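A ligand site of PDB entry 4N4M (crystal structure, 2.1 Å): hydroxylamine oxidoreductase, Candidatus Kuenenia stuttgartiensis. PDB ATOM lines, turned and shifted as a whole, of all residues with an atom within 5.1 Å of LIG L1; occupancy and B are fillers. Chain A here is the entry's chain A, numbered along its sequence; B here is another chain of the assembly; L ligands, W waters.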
ATOM      1  N   TRP A  58      -9.681   6.064 -24.757  1.00  0.00           N
ATOM      2  CA  TRP A  58      -9.124   7.358 -25.123  1.00  0.00           C
ATOM      3  C   TRP A  58     -10.195   8.353 -25.598  1.00  0.00           C
ATOM      4  O   TRP A  58      -9.994   9.558 -25.529  1.00  0.00           O
ATOM      5  CB  TRP A  58      -8.050   7.200 -26.221  1.00  0.00           C
ATOM      6  CG  TRP A  58      -6.941   6.257 -25.844  1.00  0.00           C
ATOM      7  CD1 TRP A  58      -6.858   4.924 -26.157  1.00  0.00           C
ATOM      8  CD2 TRP A  58      -5.786   6.558 -25.058  1.00  0.00           C
ATOM      9  NE1 TRP A  58      -5.712   4.387 -25.618  1.00  0.00           N
ATOM     10  CE2 TRP A  58      -5.031   5.368 -24.941  1.00  0.00           C
ATOM     11  CE3 TRP A  58      -5.292   7.717 -24.461  1.00  0.00           C
ATOM     12  CZ2 TRP A  58      -3.834   5.313 -24.239  1.00  0.00           C
ATOM     13  CZ3 TRP A  58      -4.104   7.662 -23.760  1.00  0.00           C
ATOM     14  CH2 TRP A  58      -3.379   6.470 -23.653  1.00  0.00           C
ATOM     15  N   TRP A  65     -12.008   5.089 -19.090  1.00  0.00           N
ATOM     16  CA  TRP A  65     -10.604   5.338 -18.757  1.00  0.00           C
ATOM     17  C   TRP A  65     -10.223   4.707 -17.417  1.00  0.00           C
ATOM     18  O   TRP A  65     -10.942   4.852 -16.436  1.00  0.00           O
ATOM     19  CB  TRP A  65     -10.305   6.838 -18.694  1.00  0.00           C
ATOM     20  CG  TRP A  65      -8.866   7.142 -18.405  1.00  0.00           C
ATOM     21  CD1 TRP A  65      -8.357   7.658 -17.245  1.00  0.00           C
ATOM     22  CD2 TRP A  65      -7.754   6.943 -19.288  1.00  0.00           C
ATOM     23  NE1 TRP A  65      -6.989   7.804 -17.357  1.00  0.00           N
ATOM     24  CE2 TRP A  65      -6.596   7.375 -18.603  1.00  0.00           C
ATOM     25  CE3 TRP A  65      -7.623   6.456 -20.590  1.00  0.00           C
ATOM     26  CZ2 TRP A  65      -5.330   7.320 -19.175  1.00  0.00           C
ATOM     27  CZ3 TRP A  65      -6.357   6.401 -21.162  1.00  0.00           C
ATOM     28  CH2 TRP A  65      -5.220   6.837 -20.446  1.00  0.00           C
ATOM     29  N   GLY A  68      -3.270   2.811 -16.510  1.00  0.00           N
ATOM     30  CA  GLY A  68      -2.509   1.774 -17.200  1.00  0.00           C
ATOM     31  C   GLY A  68      -1.039   2.120 -17.311  1.00  0.00           C
ATOM     32  O   GLY A  68      -0.362   1.666 -18.234  1.00  0.00           O
ATOM     33  N   SER A  69      -0.541   2.932 -16.378  1.00  0.00           N
ATOM     34  CA  SER A  69       0.840   3.377 -16.380  1.00  0.00           C
ATOM     35  C   SER A  69       1.687   2.491 -15.466  1.00  0.00           C
ATOM     36  O   SER A  69       1.185   1.901 -14.499  1.00  0.00           O
ATOM     37  CB  SER A  69       0.908   4.837 -15.922  1.00  0.00           C
ATOM     38  OG  SER A  69       2.251   5.275 -15.770  1.00  0.00           O
ATOM     39  N   GLN A  70       2.970   2.399 -15.793  1.00  0.00           N
ATOM     40  CA  GLN A  70       3.941   1.660 -14.995  1.00  0.00           C
ATOM     41  C   GLN A  70       4.825   2.614 -14.192  1.00  0.00           C
ATOM     42  O   GLN A  70       5.633   2.180 -13.377  1.00  0.00           O
ATOM     43  CB  GLN A  70       4.831   0.779 -15.881  1.00  0.00           C
ATOM     44  CG  GLN A  70       4.072  -0.355 -16.570  1.00  0.00           C
ATOM     45  CD  GLN A  70       3.150   0.130 -17.693  1.00  0.00           C
ATOM     46  OE1 GLN A  70       1.986  -0.282 -17.777  1.00  0.00           O
ATOM     47  NE2 GLN A  70       3.655   1.009 -18.545  1.00  0.00           N
ATOM     48  N   THR A  71       4.664   3.919 -14.413  1.00  0.00           N
ATOM     49  CA  THR A  71       5.445   4.937 -13.706  1.00  0.00           C
ATOM     50  C   THR A  71       4.663   5.385 -12.466  1.00  0.00           C
ATOM     51  O   THR A  71       3.471   5.674 -12.550  1.00  0.00           O
ATOM     52  CB  THR A  71       5.761   6.128 -14.632  1.00  0.00           C
ATOM     53  OG1 THR A  71       6.546   5.664 -15.734  1.00  0.00           O
ATOM     54  CG2 THR A  71       6.525   7.222 -13.882  1.00  0.00           C
ATOM     55  N   PHE A  75       4.145  14.124  -8.858  1.00  0.00           N
ATOM     56  CA  PHE A  75       5.139  15.018  -9.434  1.00  0.00           C
ATOM     57  C   PHE A  75       4.652  16.459  -9.579  1.00  0.00           C
ATOM     58  O   PHE A  75       3.459  16.718  -9.683  1.00  0.00           O
ATOM     59  CB  PHE A  75       5.563  14.505 -10.817  1.00  0.00           C
ATOM     60  CG  PHE A  75       6.160  13.123 -10.793  1.00  0.00           C
ATOM     61  CD1 PHE A  75       7.438  12.918 -10.297  1.00  0.00           C
ATOM     62  CD2 PHE A  75       5.454  12.039 -11.285  1.00  0.00           C
ATOM     63  CE1 PHE A  75       8.001  11.649 -10.269  1.00  0.00           C
ATOM     64  CE2 PHE A  75       6.008  10.767 -11.266  1.00  0.00           C
ATOM     65  CZ  PHE A  75       7.286  10.566 -10.761  1.00  0.00           C
ATOM     66  N   LYS A  76       5.600  17.381  -9.568  1.00  0.00           N
ATOM     67  CA  LYS A  76       5.360  18.790  -9.891  1.00  0.00           C
ATOM     68  C   LYS A  76       5.370  18.964 -11.406  1.00  0.00           C
ATOM     69  O   LYS A  76       5.976  18.157 -12.123  1.00  0.00           O
ATOM     70  CB  LYS A  76       6.448  19.666  -9.280  1.00  0.00           C
ATOM     71  CG  LYS A  76       6.543  19.598  -7.754  1.00  0.00           C
ATOM     72  CD  LYS A  76       7.804  20.284  -7.221  1.00  0.00           C
ATOM     73  CE  LYS A  76       7.825  20.301  -5.690  1.00  0.00           C
ATOM     74  NZ  LYS A  76       9.079  20.901  -5.129  1.00  0.00           N
ATOM     75  N   GLU A  79       8.651  18.630 -13.181  1.00  0.00           N
ATOM     76  CA  GLU A  79       9.071  17.228 -13.261  1.00  0.00           C
ATOM     77  C   GLU A  79       8.408  16.493 -14.427  1.00  0.00           C
ATOM     78  O   GLU A  79       9.042  15.681 -15.098  1.00  0.00           O
ATOM     79  CB  GLU A  79       8.815  16.504 -11.927  1.00  0.00           C
ATOM     80  CG  GLU A  79       9.707  17.035 -10.787  1.00  0.00           C
ATOM     81  CD  GLU A  79       9.406  16.428  -9.417  1.00  0.00           C
ATOM     82  OE1 GLU A  79      10.373  16.261  -8.638  1.00  0.00           O
ATOM     83  OE2 GLU A  79       8.240  16.120  -9.110  1.00  0.00           O
ATOM     84  N   CYS A  80       7.134  16.792 -14.680  1.00  0.00           N
ATOM     85  CA  CYS A  80       6.446  16.275 -15.876  1.00  0.00           C
ATOM     86  C   CYS A  80       7.246  16.608 -17.128  1.00  0.00           C
ATOM     87  O   CYS A  80       7.512  15.737 -17.955  1.00  0.00           O
ATOM     88  CB  CYS A  80       5.036  16.882 -16.026  1.00  0.00           C
ATOM     89  SG  CYS A  80       3.937  16.727 -14.595  1.00  0.00           S
ATOM     90  N   CYS A  83      11.102  14.924 -17.498  1.00  0.00           N
ATOM     91  CA  CYS A  83      11.132  13.505 -17.840  1.00  0.00           C
ATOM     92  C   CYS A  83      10.550  13.254 -19.237  1.00  0.00           C
ATOM     93  O   CYS A  83      11.120  12.479 -20.012  1.00  0.00           O
ATOM     94  CB  CYS A  83      10.372  12.676 -16.819  1.00  0.00           C
ATOM     95  SG  CYS A  83      10.575  10.883 -17.061  1.00  0.00           S
ATOM     96  N   HIS A  84       9.419  13.889 -19.546  1.00  0.00           N
ATOM     97  CA  HIS A  84       8.775  13.698 -20.839  1.00  0.00           C
ATOM     98  C   HIS A  84       9.548  14.311 -22.006  1.00  0.00           C
ATOM     99  O   HIS A  84       9.328  13.930 -23.153  1.00  0.00           O
ATOM    100  CB  HIS A  84       7.320  14.191 -20.831  1.00  0.00           C
ATOM    101  CG  HIS A  84       6.362  13.164 -20.327  1.00  0.00           C
ATOM    102  ND1 HIS A  84       5.791  12.216 -21.159  1.00  0.00           N
ATOM    103  CD2 HIS A  84       5.917  12.896 -19.086  1.00  0.00           C
ATOM    104  CE1 HIS A  84       5.018  11.432 -20.441  1.00  0.00           C
ATOM    105  NE2 HIS A  84       5.083  11.810 -19.175  1.00  0.00           N
ATOM    106  N   GLN A  87      11.070  11.135 -22.646  1.00  0.00           N
ATOM    107  CA  GLN A  87      10.160  10.004 -22.903  1.00  0.00           C
ATOM    108  C   GLN A  87       9.161  10.189 -24.050  1.00  0.00           C
ATOM    109  O   GLN A  87       8.843   9.215 -24.745  1.00  0.00           O
ATOM    110  CB  GLN A  87       9.426   9.625 -21.619  1.00  0.00           C
ATOM    111  CG  GLN A  87      10.322   8.986 -20.582  1.00  0.00           C
ATOM    112  CD  GLN A  87      10.979   7.710 -21.083  1.00  0.00           C
ATOM    113  OE1 GLN A  87      10.306   6.813 -21.590  1.00  0.00           O
ATOM    114  NE2 GLN A  87      12.303   7.639 -20.950  1.00  0.00           N
ATOM    115  N   CYS A 124       1.442  19.969 -17.744  1.00  0.00           N
ATOM    116  CA  CYS A 124       0.974  18.600 -17.889  1.00  0.00           C
ATOM    117  C   CYS A 124       0.062  18.180 -16.732  1.00  0.00           C
ATOM    118  O   CYS A 124      -0.969  17.548 -16.947  1.00  0.00           O
ATOM    119  CB  CYS A 124       2.162  17.616 -17.972  1.00  0.00           C
ATOM    120  SG  CYS A 124       3.595  18.183 -18.943  1.00  0.00           S
ATOM    121  N   ALA A 125       0.479  18.532 -15.514  1.00  0.00           N
ATOM    122  CA  ALA A 125      -0.243  18.134 -14.297  1.00  0.00           C
ATOM    123  C   ALA A 125      -1.590  18.851 -14.155  1.00  0.00           C
ATOM    124  O   ALA A 125      -2.543  18.279 -13.609  1.00  0.00           O
ATOM    125  CB  ALA A 125       0.618  18.392 -13.061  1.00  0.00           C
ATOM    126  N   HIS A 128      -3.709  16.749 -16.654  1.00  0.00           N
ATOM    127  CA  HIS A 128      -3.714  15.296 -16.502  1.00  0.00           C
ATOM    128  C   HIS A 128      -3.680  14.805 -15.056  1.00  0.00           C
ATOM    129  O   HIS A 128      -3.934  13.631 -14.812  1.00  0.00           O
ATOM    130  CB  HIS A 128      -2.532  14.696 -17.265  1.00  0.00           C
ATOM    131  CG  HIS A 128      -2.657  14.804 -18.754  1.00  0.00           C
ATOM    132  ND1 HIS A 128      -3.543  14.039 -19.475  1.00  0.00           N
ATOM    133  CD2 HIS A 128      -1.997  15.574 -19.653  1.00  0.00           C
ATOM    134  CE1 HIS A 128      -3.435  14.338 -20.759  1.00  0.00           C
ATOM    135  NE2 HIS A 128      -2.500  15.264 -20.892  1.00  0.00           N
ATOM    136  N   GLY A 129      -3.390  15.682 -14.112  1.00  0.00           N
ATOM    137  CA  GLY A 129      -3.218  15.293 -12.707  1.00  0.00           C
ATOM    138  C   GLY A 129      -1.752  15.135 -12.293  1.00  0.00           C
ATOM    139  O   GLY A 129      -0.876  15.046 -13.142  1.00  0.00           O
ATOM    140  N   ASN A 130      -1.515  15.084 -10.979  1.00  0.00           N
ATOM    141  CA  ASN A 130      -0.171  15.031 -10.396  1.00  0.00           C
ATOM    142  C   ASN A 130       0.310  13.617 -10.088  1.00  0.00           C
ATOM    143  O   ASN A 130       1.515  13.372 -10.001  1.00  0.00           O
ATOM    144  CB  ASN A 130      -0.134  15.826  -9.083  1.00  0.00           C
ATOM    145  CG  ASN A 130      -0.274  17.309  -9.293  1.00  0.00           C
ATOM    146  OD1 ASN A 130      -1.370  17.876  -9.147  1.00  0.00           O
ATOM    147  ND2 ASN A 130       0.825  17.977  -9.639  1.00  0.00           N
ATOM    148  N   HIS A 132       0.933   9.926 -11.078  1.00  0.00           N
ATOM    149  CA  HIS A 132       1.166   9.183 -12.321  1.00  0.00           C
ATOM    150  C   HIS A 132       0.445   7.833 -12.370  1.00  0.00           C
ATOM    151  O   HIS A 132       0.414   7.193 -13.423  1.00  0.00           O
ATOM    152  CB  HIS A 132       2.661   8.994 -12.580  1.00  0.00           C
ATOM    153  CG  HIS A 132       3.018   8.969 -14.034  1.00  0.00           C
ATOM    154  ND1 HIS A 132       2.701   7.913 -14.868  1.00  0.00           N
ATOM    155  CD2 HIS A 132       3.622   9.893 -14.816  1.00  0.00           C
ATOM    156  CE1 HIS A 132       3.105   8.182 -16.089  1.00  0.00           C
ATOM    157  NE2 HIS A 132       3.669   9.383 -16.087  1.00  0.00           N
ATOM    158  N   LEU A 135      -3.599   9.261 -13.485  1.00  0.00           N
ATOM    159  CA  LEU A 135      -3.589  10.259 -14.562  1.00  0.00           C
ATOM    160  C   LEU A 135      -4.959  10.313 -15.223  1.00  0.00           C
ATOM    161  O   LEU A 135      -5.637   9.296 -15.351  1.00  0.00           O
ATOM    162  CB  LEU A 135      -2.518   9.914 -15.612  1.00  0.00           C
ATOM    163  CG  LEU A 135      -1.058  10.037 -15.157  1.00  0.00           C
ATOM    164  CD1 LEU A 135      -0.103   9.443 -16.199  1.00  0.00           C
ATOM    165  CD2 LEU A 135      -0.683  11.491 -14.832  1.00  0.00           C
ATOM    166  N   MET A 137      -7.485  11.448 -18.525  1.00  0.00           N
ATOM    167  CA  MET A 137      -7.557  11.653 -19.957  1.00  0.00           C
ATOM    168  C   MET A 137      -8.798  12.540 -20.160  1.00  0.00           C
ATOM    169  O   MET A 137      -9.926  12.076 -20.002  1.00  0.00           O
ATOM    170  CB  MET A 137      -7.697  10.300 -20.659  1.00  0.00           C
ATOM    171  CG  MET A 137      -7.280  10.281 -22.114  1.00  0.00           C
ATOM    172  SD  MET A 137      -5.702  11.082 -22.442  1.00  0.00           S
ATOM    173  CE  MET A 137      -4.581  10.229 -21.351  1.00  0.00           C
ATOM    174  N   GLN B 311       6.334   6.387 -29.727  1.00  0.00           N
ATOM    175  CA  GLN B 311       6.566   7.051 -28.452  1.00  0.00           C
ATOM    176  C   GLN B 311       7.431   8.304 -28.576  1.00  0.00           C
ATOM    177  O   GLN B 311       7.524   9.080 -27.625  1.00  0.00           O
ATOM    178  CB  GLN B 311       7.172   6.083 -27.420  1.00  0.00           C
ATOM    179  CG  GLN B 311       7.001   6.528 -25.970  1.00  0.00           C
ATOM    180  CD  GLN B 311       7.681   5.607 -24.967  1.00  0.00           C
ATOM    181  OE1 GLN B 311       7.717   4.395 -25.160  1.00  0.00           O
ATOM    182  NE2 GLN B 311       8.228   6.175 -23.906  1.00  0.00           N
ATOM    183  N   SER B 315       2.119   8.556 -25.933  1.00  0.00           N
ATOM    184  CA  SER B 315       2.108   7.487 -24.946  1.00  0.00           C
ATOM    185  C   SER B 315       2.269   6.139 -25.633  1.00  0.00           C
ATOM    186  O   SER B 315       1.618   5.884 -26.647  1.00  0.00           O
ATOM    187  CB  SER B 315       0.780   7.492 -24.200  1.00  0.00           C
ATOM    188  OG  SER B 315       0.526   6.218 -23.630  1.00  0.00           O
ATOM    189  N   PRO B 316       3.100   5.251 -25.056  1.00  0.00           N
ATOM    190  CA  PRO B 316       3.246   3.910 -25.626  1.00  0.00           C
ATOM    191  C   PRO B 316       1.993   3.042 -25.492  1.00  0.00           C
ATOM    192  O   PRO B 316       1.802   2.110 -26.268  1.00  0.00           O
ATOM    193  CB  PRO B 316       4.416   3.308 -24.829  1.00  0.00           C
ATOM    194  CG  PRO B 316       4.412   4.053 -23.539  1.00  0.00           C
ATOM    195  CD  PRO B 316       3.939   5.440 -23.856  1.00  0.00           C
ATOM    196  N   ARG B 317       1.154   3.350 -24.508  1.00  0.00           N
ATOM    197  CA  ARG B 317      -0.102   2.632 -24.308  1.00  0.00           C
ATOM    198  C   ARG B 317      -1.093   2.968 -25.433  1.00  0.00           C
ATOM    199  O   ARG B 317      -1.774   2.082 -25.967  1.00  0.00           O
ATOM    200  CB  ARG B 317      -0.673   3.015 -22.949  1.00  0.00           C
ATOM    201  CG  ARG B 317      -1.913   2.252 -22.521  1.00  0.00           C
ATOM    202  CD  ARG B 317      -2.566   2.964 -21.350  1.00  0.00           C
ATOM    203  NE  ARG B 317      -3.753   2.279 -20.858  1.00  0.00           N
ATOM    204  CZ  ARG B 317      -4.569   2.755 -19.936  1.00  0.00           C
ATOM    205  NH1 ARG B 317      -4.352   3.950 -19.382  1.00  0.00           N
ATOM    206  NH2 ARG B 317      -5.622   2.051 -19.563  1.00  0.00           N
ATOM    207  N   PHE B 318      -1.170   4.248 -25.773  1.00  0.00           N
ATOM    208  CA  PHE B 318      -1.961   4.712 -26.917  1.00  0.00           C
ATOM    209  C   PHE B 318      -1.509   4.064 -28.230  1.00  0.00           C
ATOM    210  O   PHE B 318      -2.329   3.530 -28.985  1.00  0.00           O
ATOM    211  CB  PHE B 318      -1.843   6.241 -27.023  1.00  0.00           C
ATOM    212  CG  PHE B 318      -2.575   6.830 -28.199  1.00  0.00           C
ATOM    213  CD1 PHE B 318      -3.952   6.713 -28.295  1.00  0.00           C
ATOM    214  CD2 PHE B 318      -1.887   7.500 -29.196  1.00  0.00           C
ATOM    215  CE1 PHE B 318      -4.631   7.258 -29.385  1.00  0.00           C
ATOM    216  CE2 PHE B 318      -2.556   8.048 -30.276  1.00  0.00           C
ATOM    217  CZ  PHE B 318      -3.932   7.932 -30.373  1.00  0.00           C
HETATM  218 FE1  LIG L   1       4.408  10.653 -17.584  1.00  0.00          FE
HETATM  219  C1  LIG L   1       3.120   8.191 -19.648  1.00  0.00           C
HETATM  220  C2  LIG L   1       1.553  12.435 -17.914  1.00  0.00           C
HETATM  221  C3  LIG L   1       5.530  12.914 -15.230  1.00  0.00           C
HETATM  222  C4  LIG L   1       7.428   9.086 -17.509  1.00  0.00           C
HETATM  223  N1  LIG L   1       2.698  10.401 -18.687  1.00  0.00           N
HETATM  224  C5  LIG L   1       2.297   9.253 -19.319  1.00  0.00           C
HETATM  225  C6  LIG L   1       0.923   9.446 -19.735  1.00  0.00           C
HETATM  226  C7  LIG L   1       0.503  10.625 -19.285  1.00  0.00           C
HETATM  227  C8  LIG L   1       1.612  11.249 -18.597  1.00  0.00           C
HETATM  228  C9  LIG L   1      -0.729  11.404 -19.812  1.00  0.00           C
HETATM  229  C10 LIG L   1       0.065   8.426 -20.509  1.00  0.00           C
HETATM  230  C11 LIG L   1      -0.445   7.387 -19.522  1.00  0.00           C
HETATM  231  C12 LIG L   1      -1.182   6.289 -20.226  1.00  0.00           C
HETATM  232  O1  LIG L   1      -0.726   5.866 -21.320  1.00  0.00           O
HETATM  233  O2  LIG L   1      -2.164   5.758 -19.644  1.00  0.00           O
HETATM  234  N2  LIG L   1       3.680  12.361 -16.727  1.00  0.00           N
HETATM  235  C13 LIG L   1       2.427  12.864 -16.960  1.00  0.00           C
HETATM  236  C14 LIG L   1       2.246  14.010 -16.087  1.00  0.00           C
HETATM  237  C15 LIG L   1       3.281  14.033 -15.237  1.00  0.00           C
HETATM  238  C16 LIG L   1       4.297  13.161 -15.798  1.00  0.00           C
HETATM  239  C17 LIG L   1       0.995  14.910 -16.034  1.00  0.00           C
HETATM  240  C18 LIG L   1       3.512  15.060 -14.108  1.00  0.00           C
HETATM  241  C19 LIG L   1       2.630  15.159 -13.111  1.00  0.00           C
HETATM  242  N3  LIG L   1       6.105  10.877 -16.471  1.00  0.00           N
HETATM  243  C20 LIG L   1       6.411  11.934 -15.637  1.00  0.00           C
HETATM  244  C21 LIG L   1       7.700  11.655 -15.032  1.00  0.00           C
HETATM  245  C22 LIG L   1       8.250  10.628 -15.687  1.00  0.00           C
HETATM  246  C23 LIG L   1       7.236  10.091 -16.586  1.00  0.00           C
HETATM  247  C24 LIG L   1       8.306  12.446 -13.848  1.00  0.00           C
HETATM  248  C25 LIG L   1       9.734  10.170 -15.634  1.00  0.00           C
HETATM  249  C26 LIG L   1      10.429  10.259 -14.491  1.00  0.00           C
HETATM  250  N4  LIG L   1       5.163   8.898 -18.443  1.00  0.00           N
HETATM  251  C27 LIG L   1       6.446   8.419 -18.198  1.00  0.00           C
HETATM  252  C28 LIG L   1       6.674   7.249 -19.016  1.00  0.00           C
HETATM  253  C29 LIG L   1       5.293   6.893 -19.565  1.00  0.00           C
HETATM  254  C30 LIG L   1       4.435   8.025 -19.256  1.00  0.00           C
HETATM  255  C31 LIG L   1       7.875   6.281 -18.931  1.00  0.00           C
HETATM  256  C32 LIG L   1       4.973   5.699 -20.491  1.00  0.00           C
HETATM  257  C33 LIG L   1       5.068   4.381 -19.731  1.00  0.00           C
HETATM  258  C34 LIG L   1       4.201   4.426 -18.503  1.00  0.00           C
HETATM  259  O3  LIG L   1       4.750   4.245 -17.378  1.00  0.00           O
HETATM  260  O4  LIG L   1       3.006   4.798 -18.623  1.00  0.00           O
HETATM  261 FE1  LG2 L   2      -1.777  16.050 -22.702  1.00  0.00          FE
HETATM  262  C1  LG2 L   2      -3.580  13.487 -24.165  1.00  0.00           C
HETATM  263  C2  LG2 L   2       0.809  13.946 -22.184  1.00  0.00           C
HETATM  264  C3  LG2 L   2       0.096  18.650 -21.396  1.00  0.00           C
HETATM  265  C4  LG2 L   2      -4.460  18.067 -22.759  1.00  0.00           C
HETATM  266  N1  LG2 L   2      -1.374  14.140 -23.304  1.00  0.00           N
HETATM  267  C5  LG2 L   2      -2.280  13.215 -23.792  1.00  0.00           C
HETATM  268  C6  LG2 L   2      -1.563  11.983 -24.006  1.00  0.00           C
HETATM  269  C7  LG2 L   2      -0.415  12.076 -23.325  1.00  0.00           C
HETATM  270  C8  LG2 L   2      -0.306  13.432 -22.822  1.00  0.00           C
HETATM  271  C9  LG2 L   2       0.712  11.024 -23.272  1.00  0.00           C
HETATM  272  C10 LG2 L   2      -2.175  10.698 -24.615  1.00  0.00           C
HETATM  273  C11 LG2 L   2      -2.387  10.839 -26.120  1.00  0.00           C
HETATM  274  C12 LG2 L   2      -1.062  10.794 -26.860  1.00  0.00           C
HETATM  275  O1  LG2 L   2      -0.931  11.500 -27.906  1.00  0.00           O
HETATM  276  O2  LG2 L   2      -0.239   9.894 -26.540  1.00  0.00           O
HETATM  277  N2  LG2 L   2       0.073  16.252 -21.892  1.00  0.00           N
HETATM  278  C13 LG2 L   2       0.964  15.219 -21.687  1.00  0.00           C
HETATM  279  C14 LG2 L   2       2.223  15.791 -21.267  1.00  0.00           C
HETATM  280  C15 LG2 L   2       2.056  17.112 -21.125  1.00  0.00           C
HETATM  281  C16 LG2 L   2       0.687  17.418 -21.481  1.00  0.00           C
HETATM  282  C17 LG2 L   2       3.477  14.992 -20.808  1.00  0.00           C
HETATM  283  C18 LG2 L   2       3.130  18.120 -20.691  1.00  0.00           C
HETATM  284  C19 LG2 L   2       4.149  18.394 -21.532  1.00  0.00           C
HETATM  285  N3  LG2 L   2      -2.132  17.947 -22.072  1.00  0.00           N
HETATM  286  C20 LG2 L   2      -1.232  18.889 -21.646  1.00  0.00           C
HETATM  287  C21 LG2 L   2      -1.953  20.113 -21.352  1.00  0.00           C
HETATM  288  C22 LG2 L   2      -3.246  19.851 -21.493  1.00  0.00           C
HETATM  289  C23 LG2 L   2      -3.383  18.516 -22.028  1.00  0.00           C
HETATM  290  C24 LG2 L   2      -1.331  21.394 -20.751  1.00  0.00           C
HETATM  291  C25 LG2 L   2      -4.405  20.821 -21.185  1.00  0.00           C
HETATM  292  C26 LG2 L   2      -4.367  22.079 -21.654  1.00  0.00           C
HETATM  293  N4  LG2 L   2      -3.667  15.855 -23.506  1.00  0.00           N
HETATM  294  C27 LG2 L   2      -4.655  16.795 -23.236  1.00  0.00           C
HETATM  295  C28 LG2 L   2      -5.928  16.307 -23.692  1.00  0.00           C
HETATM  296  C29 LG2 L   2      -5.634  14.918 -24.271  1.00  0.00           C
HETATM  297  C30 LG2 L   2      -4.236  14.692 -24.003  1.00  0.00           C
HETATM  298  C31 LG2 L   2      -7.210  17.123 -23.941  1.00  0.00           C
HETATM  299  C32 LG2 L   2      -6.684  13.914 -24.794  1.00  0.00           C
HETATM  300  C33 LG2 L   2      -6.573  13.772 -26.311  1.00  0.00           C
HETATM  301  C34 LG2 L   2      -7.159  14.956 -27.044  1.00  0.00           C
HETATM  302  O3  LG2 L   2      -6.687  15.260 -28.170  1.00  0.00           O
HETATM  303  O4  LG2 L   2      -8.159  15.547 -26.547  1.00  0.00           O
HETATM  304  O   HOH W   1      -2.699   5.623 -16.925  1.00  0.00           O
HETATM  305  O   HOH W   2       1.701   4.639 -20.750  1.00  0.00           O
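The side-chain hydroxyl of Ser 69 is in hydrogen-bond range of a ring nitrogen (ND1) of His 132, at 2.8 Å. N of Arg 317 of chain B sits at hydrogen-bond distance from OG of Ser 315 of chain B, at 3.1 Å. OG of Ser 315 of chain B lies within hydrogen-bond range of N of Phe 318 of chain B, at 3.4 Å. The backbone NH (N) of Thr 71 lies within hydrogen-bond range of the side-chain hydroxyl (OG) of Ser 69, at 3.1 Å. O of Gly 68 sits close to OE1 of Gln 70. The side-chain carboxylate (OE2) of Glu 79 is in hydrogen-bond range of the backbone NH (N) of Lys 76, 3.0 Å away. The side-chain amide nitrogen (NE2) of Gln 311 of chain B lies within hydrogen-bond range of the side-chain amide oxygen (OE1) of Gln 87 (3.2 Å). The backbone carbonyl oxygen (O) of Phe 75 is in hydrogen-bond range of the side-chain amide nitrogen (ND2) of Asn 130, at 2.9 Å.
The side-chain sulfur (SG) of Cys 80 is bonded to a carbon (C18) of LIG L1 (1.8 Å). A carbon (C25) of LIG L1 is bonded to the side-chain sulfur of Cys 83, at 1.8 Å. A ring nitrogen (NE2) of His 84 binds an iron atom (FE1) of LIG L1 (2.1 Å). An iron atom (FE1) of LIG L1 is bound by a ring nitrogen (NE2) of His 132. The side-chain hydroxyl of Ser 315 of chain B is in hydrogen-bond range of an oxygen (O1) of LIG L1 (2.7 Å). An oxygen (O3) of LIG L1 lies within hydrogen-bond range of the backbone NH (N) of Thr 71 (3.0 Å). OG1 of Thr 71 sits at hydrogen-bond distance from O3 of LIG L1, at 2.8 Å. NH1 of Arg 317 of chain B is in salt-bridge range of O2 of LIG L1. O4 of LIG L1 is in hydrogen-bond range of OG of Ser 69 (3.0 Å). An oxygen (O3) of LIG L1 lies within hydrogen-bond range of the backbone NH (N) of Gln 70, 3.0 Å away. The backbone NH (N) of Ser 315 of chain B is in hydrogen-bond range of an oxygen (O2) of LG2 L2. A carbon (C18) of LG2 L2 is covalently linked to the side-chain sulfur of Cys 124, 1.8 Å away. A ring nitrogen (NE2) of His 128 is bound to an iron atom (FE1) of LG2 L2 (2.1 Å).
Trp 58 touches LIG L1 (CH2 to O1, 3.6 Å). CH2 of Trp 65 touches O2 of LIG L1, at 3.3 Å. Phe 75 touches LIG L1. O of Glu 79 touches C24 of LIG L1 (3.5 Å). OE1 of Gln 87 touches C31 of LIG L1 (3.6 Å). Cys 124 touches LIG L1 (O to C17, 3.4 Å). Ala 125 touches LIG L1 (N to C17, 3.7 Å). CB of His 128 touches C17 of LIG L1, at 3.7 Å. Gly 129 touches LIG L1. Asn 130 touches LIG L1. Leu 135 touches LIG L1 (CD1 to C7, 3.4 Å). Pro 316 of chain B touches LIG L1 (CG to C32, 3.5 Å). Hydrophobic or aromatic side chains that line LIG L1: Trp 58, Trp 65, Phe 75, His 84, Ala 125, His 128, His 132, Leu 135 and Pro 316 of chain B. The nearest printed residue that does not touch LIG L1 is Met 137 (4.3 Å).
Water W2 lies within hydrogen-bond range of an oxygen (O4) of LIG L1 (2.5 Å) and the side-chain hydroxyl (OG) of Ser 315 of chain B (3.5 Å).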
